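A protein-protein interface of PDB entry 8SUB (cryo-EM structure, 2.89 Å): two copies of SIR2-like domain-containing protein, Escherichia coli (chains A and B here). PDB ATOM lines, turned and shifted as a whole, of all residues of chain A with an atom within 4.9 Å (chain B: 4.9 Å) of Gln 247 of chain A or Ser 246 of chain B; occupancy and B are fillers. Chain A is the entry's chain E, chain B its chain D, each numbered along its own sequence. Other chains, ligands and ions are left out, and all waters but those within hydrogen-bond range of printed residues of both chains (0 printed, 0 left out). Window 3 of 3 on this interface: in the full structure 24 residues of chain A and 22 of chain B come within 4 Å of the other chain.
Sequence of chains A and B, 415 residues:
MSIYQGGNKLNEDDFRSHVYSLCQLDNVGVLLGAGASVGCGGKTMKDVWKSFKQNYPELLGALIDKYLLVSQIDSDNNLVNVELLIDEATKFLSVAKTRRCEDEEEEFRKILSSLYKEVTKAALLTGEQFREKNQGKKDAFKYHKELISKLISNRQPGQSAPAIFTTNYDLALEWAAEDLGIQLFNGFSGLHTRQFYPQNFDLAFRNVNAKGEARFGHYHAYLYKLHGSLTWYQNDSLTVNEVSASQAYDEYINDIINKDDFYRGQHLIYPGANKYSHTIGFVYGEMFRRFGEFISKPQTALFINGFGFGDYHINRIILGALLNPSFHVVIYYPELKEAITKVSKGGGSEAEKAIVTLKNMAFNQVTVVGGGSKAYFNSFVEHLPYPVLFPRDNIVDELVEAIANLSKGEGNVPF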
ATOM      1  N   VAL A 243      -3.345  26.955  32.102  1.00  0.00           N
ATOM      2  CA  VAL A 243      -2.545  27.882  31.320  1.00  0.00           C
ATOM      3  C   VAL A 243      -3.480  28.876  30.644  1.00  0.00           C
ATOM      4  O   VAL A 243      -4.685  28.875  30.869  1.00  0.00           O
ATOM      5  CB  VAL A 243      -1.655  27.166  30.284  1.00  0.00           C
ATOM      6  CG1 VAL A 243      -0.511  26.461  30.969  1.00  0.00           C
ATOM      7  CG2 VAL A 243      -2.463  26.181  29.478  1.00  0.00           C
ATOM      8  N   SER A 244      -2.901  29.745  29.832  1.00  0.00           N
ATOM      9  CA  SER A 244      -3.661  30.704  29.048  1.00  0.00           C
ATOM     10  C   SER A 244      -3.956  30.132  27.666  1.00  0.00           C
ATOM     11  O   SER A 244      -3.372  29.132  27.248  1.00  0.00           O
ATOM     12  CB  SER A 244      -2.893  32.018  28.942  1.00  0.00           C
ATOM     13  OG  SER A 244      -3.502  32.886  28.020  1.00  0.00           O
ATOM     14  N   ALA A 245      -4.883  30.782  26.955  1.00  0.00           N
ATOM     15  CA  ALA A 245      -5.335  30.259  25.666  1.00  0.00           C
ATOM     16  C   ALA A 245      -4.207  30.227  24.639  1.00  0.00           C
ATOM     17  O   ALA A 245      -4.065  29.252  23.890  1.00  0.00           O
ATOM     18  CB  ALA A 245      -6.505  31.090  25.153  1.00  0.00           C
ATOM     19  N   SER A 246      -3.390  31.282  24.593  1.00  0.00           N
ATOM     20  CA  SER A 246      -2.247  31.305  23.688  1.00  0.00           C
ATOM     21  C   SER A 246      -1.287  30.168  23.993  1.00  0.00           C
ATOM     22  O   SER A 246      -0.810  29.473  23.086  1.00  0.00           O
ATOM     23  CB  SER A 246      -1.514  32.638  23.817  1.00  0.00           C
ATOM     24  OG  SER A 246      -2.346  33.721  23.458  1.00  0.00           O
ATOM     25  N   GLN A 247      -1.002  29.962  25.275  1.00  0.00           N
ATOM     26  CA  GLN A 247      -0.046  28.944  25.678  1.00  0.00           C
ATOM     27  C   GLN A 247      -0.566  27.543  25.386  1.00  0.00           C
ATOM     28  O   GLN A 247       0.183  26.688  24.900  1.00  0.00           O
ATOM     29  CB  GLN A 247       0.273  29.121  27.157  1.00  0.00           C
ATOM     30  CG  GLN A 247       1.564  28.487  27.596  1.00  0.00           C
ATOM     31  CD  GLN A 247       1.975  28.948  28.968  1.00  0.00           C
ATOM     32  OE1 GLN A 247       1.510  29.978  29.448  1.00  0.00           O
ATOM     33  NE2 GLN A 247       2.838  28.183  29.617  1.00  0.00           N
ATOM     34  N   ALA A 248      -1.847  27.285  25.667  1.00  0.00           N
ATOM     35  CA  ALA A 248      -2.421  25.978  25.363  1.00  0.00           C
ATOM     36  C   ALA A 248      -2.410  25.707  23.867  1.00  0.00           C
ATOM     37  O   ALA A 248      -2.094  24.592  23.429  1.00  0.00           O
ATOM     38  CB  ALA A 248      -3.844  25.886  25.914  1.00  0.00           C
ATOM     39  N   TYR A 249      -2.754  26.720  23.067  1.00  0.00           N
ATOM     40  CA  TYR A 249      -2.730  26.566  21.619  1.00  0.00           C
ATOM     41  C   TYR A 249      -1.333  26.230  21.122  1.00  0.00           C
ATOM     42  O   TYR A 249      -1.166  25.365  20.257  1.00  0.00           O
ATOM     43  CB  TYR A 249      -3.239  27.843  20.958  1.00  0.00           C
ATOM     44  CG  TYR A 249      -3.453  27.727  19.474  1.00  0.00           C
ATOM     45  CD1 TYR A 249      -2.421  27.969  18.586  1.00  0.00           C
ATOM     46  CD2 TYR A 249      -4.693  27.389  18.958  1.00  0.00           C
ATOM     47  CE1 TYR A 249      -2.612  27.868  17.235  1.00  0.00           C
ATOM     48  CE2 TYR A 249      -4.893  27.286  17.607  1.00  0.00           C
ATOM     49  CZ  TYR A 249      -3.848  27.527  16.751  1.00  0.00           C
ATOM     50  OH  TYR A 249      -4.037  27.427  15.394  1.00  0.00           O
ATOM     51  N   ASP A 250      -0.313  26.903  21.654  1.00  0.00           N
ATOM     52  CA  ASP A 250       1.043  26.619  21.203  1.00  0.00           C
ATOM     53  C   ASP A 250       1.598  25.323  21.781  1.00  0.00           C
ATOM     54  O   ASP A 250       2.571  24.789  21.241  1.00  0.00           O
ATOM     55  CB  ASP A 250       1.962  27.787  21.553  1.00  0.00           C
ATOM     56  CG  ASP A 250       1.799  28.959  20.604  1.00  0.00           C
ATOM     57  OD1 ASP A 250       1.630  28.726  19.389  1.00  0.00           O
ATOM     58  OD2 ASP A 250       1.840  30.117  21.067  1.00  0.00           O
ATOM     59  N   GLU A 251       1.006  24.799  22.856  1.00  0.00           N
ATOM     60  CA  GLU A 251       1.509  23.578  23.483  1.00  0.00           C
ATOM     61  C   GLU A 251       0.909  22.311  22.881  1.00  0.00           C
ATOM     62  O   GLU A 251       1.650  21.419  22.459  1.00  0.00           O
ATOM     63  CB  GLU A 251       1.256  23.616  24.992  1.00  0.00           C
ATOM     64  CG  GLU A 251       2.379  24.243  25.784  1.00  0.00           C
ATOM     65  CD  GLU A 251       2.085  24.298  27.268  1.00  0.00           C
ATOM     66  OE1 GLU A 251       1.071  23.711  27.697  1.00  0.00           O
ATOM     67  OE2 GLU A 251       2.865  24.936  28.006  1.00  0.00           O
ATOM     68  N   ARG B 131      12.377  29.098  31.819  1.00  0.00           N
ATOM     69  CA  ARG B 131      11.084  28.801  31.220  1.00  0.00           C
ATOM     70  C   ARG B 131      10.442  27.533  31.771  1.00  0.00           C
ATOM     71  O   ARG B 131       9.398  27.115  31.267  1.00  0.00           O
ATOM     72  CB  ARG B 131      11.223  28.689  29.704  1.00  0.00           C
ATOM     73  CG  ARG B 131      12.167  27.603  29.250  1.00  0.00           C
ATOM     74  CD  ARG B 131      12.246  27.557  27.737  1.00  0.00           C
ATOM     75  NE  ARG B 131      10.936  27.369  27.123  1.00  0.00           N
ATOM     76  CZ  ARG B 131      10.303  26.206  27.046  1.00  0.00           C
ATOM     77  NH1 ARG B 131      10.843  25.092  27.514  1.00  0.00           N
ATOM     78  NH2 ARG B 131       9.102  26.157  26.481  1.00  0.00           N
ATOM     79  N   SER B 244       3.191  35.289  31.915  1.00  0.00           N
ATOM     80  CA  SER B 244       3.987  34.306  32.633  1.00  0.00           C
ATOM     81  C   SER B 244       5.406  34.253  32.074  1.00  0.00           C
ATOM     82  O   SER B 244       5.729  34.871  31.058  1.00  0.00           O
ATOM     83  CB  SER B 244       3.338  32.928  32.559  1.00  0.00           C
ATOM     84  OG  SER B 244       3.591  32.316  31.313  1.00  0.00           O
ATOM     85  N   ALA B 245       6.264  33.488  32.749  1.00  0.00           N
ATOM     86  CA  ALA B 245       7.681  33.445  32.427  1.00  0.00           C
ATOM     87  C   ALA B 245       8.016  32.543  31.247  1.00  0.00           C
ATOM     88  O   ALA B 245       9.138  32.616  30.742  1.00  0.00           O
ATOM     89  CB  ALA B 245       8.480  32.997  33.645  1.00  0.00           C
ATOM     90  N   SER B 246       7.093  31.691  30.806  1.00  0.00           N
ATOM     91  CA  SER B 246       7.310  30.868  29.622  1.00  0.00           C
ATOM     92  C   SER B 246       6.937  31.602  28.342  1.00  0.00           C
ATOM     93  O   SER B 246       7.680  31.551  27.355  1.00  0.00           O
ATOM     94  CB  SER B 246       6.502  29.575  29.721  1.00  0.00           C
ATOM     95  OG  SER B 246       6.894  28.817  30.849  1.00  0.00           O
ATOM     96  N   GLN B 247       5.789  32.278  28.345  1.00  0.00           N
ATOM     97  CA  GLN B 247       5.392  33.065  27.186  1.00  0.00           C
ATOM     98  C   GLN B 247       6.373  34.198  26.928  1.00  0.00           C
ATOM     99  O   GLN B 247       6.684  34.502  25.773  1.00  0.00           O
ATOM    100  CB  GLN B 247       3.996  33.635  27.387  1.00  0.00           C
ATOM    101  CG  GLN B 247       2.840  32.733  27.076  1.00  0.00           C
ATOM    102  CD  GLN B 247       1.532  33.485  27.152  1.00  0.00           C
ATOM    103  OE1 GLN B 247       1.491  34.703  27.011  1.00  0.00           O
ATOM    104  NE2 GLN B 247       0.449  32.759  27.372  1.00  0.00           N
ATOM    105  N   ALA B 248       6.857  34.847  27.988  1.00  0.00           N
ATOM    106  CA  ALA B 248       7.810  35.940  27.819  1.00  0.00           C
ATOM    107  C   ALA B 248       9.074  35.463  27.118  1.00  0.00           C
ATOM    108  O   ALA B 248       9.569  36.113  26.189  1.00  0.00           O
ATOM    109  CB  ALA B 248       8.147  36.546  29.179  1.00  0.00           C
ATOM    110  N   TYR B 249       9.601  34.316  27.544  1.00  0.00           N
ATOM    111  CA  TYR B 249      10.789  33.755  26.914  1.00  0.00           C
ATOM    112  C   TYR B 249      10.512  33.367  25.470  1.00  0.00           C
ATOM    113  O   TYR B 249      11.286  33.698  24.566  1.00  0.00           O
ATOM    114  CB  TYR B 249      11.265  32.544  27.709  1.00  0.00           C
ATOM    115  CG  TYR B 249      12.607  31.999  27.292  1.00  0.00           C
ATOM    116  CD1 TYR B 249      12.720  31.075  26.265  1.00  0.00           C
ATOM    117  CD2 TYR B 249      13.762  32.392  27.948  1.00  0.00           C
ATOM    118  CE1 TYR B 249      13.946  30.573  25.895  1.00  0.00           C
ATOM    119  CE2 TYR B 249      14.990  31.896  27.585  1.00  0.00           C
ATOM    120  CZ  TYR B 249      15.078  30.985  26.561  1.00  0.00           C
ATOM    121  OH  TYR B 249      16.308  30.489  26.200  1.00  0.00           O
ATOM    122  N   ASP B 250       9.404  32.664  25.229  1.00  0.00           N
ATOM    123  CA  ASP B 250       9.107  32.214  23.876  1.00  0.00           C
ATOM    124  C   ASP B 250       8.715  33.358  22.954  1.00  0.00           C
ATOM    125  O   ASP B 250       8.675  33.165  21.736  1.00  0.00           O
ATOM    126  CB  ASP B 250       7.992  31.169  23.902  1.00  0.00           C
ATOM    127  CG  ASP B 250       8.466  29.820  24.419  1.00  0.00           C
ATOM    128  OD1 ASP B 250       9.656  29.491  24.238  1.00  0.00           O
ATOM    129  OD2 ASP B 250       7.644  29.083  25.003  1.00  0.00           O
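The side-chain hydroxyl (OG) of Ser 246 of chain B is in hydrogen-bond range of the backbone carbonyl oxygen (O) of Arg 131 of chain B (3.1 Å).
NE2 of Gln 247 of chain B touches CB of Ser 244 of chain A, at 3.8 Å.
OE1 of Gln 247 of chain A touches OG of Ser 244 of chain B, 3.6 Å away.
Gln 247 of chain A touches Ser 246 of chain B.
Gln 247 of chain B touches Gln 247 of chain A.
Gln 247 of chain A touches just these residues of chain B: Ser 244 (3.6 Å), Ser 246 (3.9 Å) and Gln 247 (3.6 Å).
Of the printed residues of chain A, Ser 246 of chain B touches Gln 247 (3.9 Å).
Of the printed residues of chain A, Ser 244 of chain B touches Gln 247.
Of the printed residues of chain B, Ser 244 of chain A touches Gln 247 (3.8 Å).
Printed residues of chain A within 4 Å of Gln 247 of chain B: Ser 244 and Gln 247.
Ala 248 of chain A touches none of the printed residues of chain B.
The nearest printed residue of chain B that does not touch Gln 247 of chain A is Asp 250 of chain B (6.6 Å).
The nearest printed residue of chain A that does not touch Ser 244 of chain B is Ser 244 of chain A (6.9 Å).
Printed residues of chain B that touch a printed residue of chain A: Ser 244, Ser 246 and Gln 247.
Printed residues of chain A that touch a printed residue of chain B: Ser 244 and Gln 247.
Among the printed residues, 4 pairs touch across the chains.
Among the printed residues, no Asp or Glu carboxylate lies within 4 Å of a Lys or Arg side-chain nitrogen of the other chain.
Ser 244 of chain A touches Gln 247 of chain B, and with the chains exchanged Gln 247 of chain A touches Ser 244 of chain B.
Gln 247 of chain A touches Ser 246 of chain B, but with the chains exchanged Ser 246 of chain A does not touch Gln 247 of chain B (4.1 Å).
Gln 247 of chain B touches its own counterpart, Gln 247 of chain A.
Of the 4 pairs that touch across the chains among the printed residues, 3 have their exchanged pair printed and touching as well.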
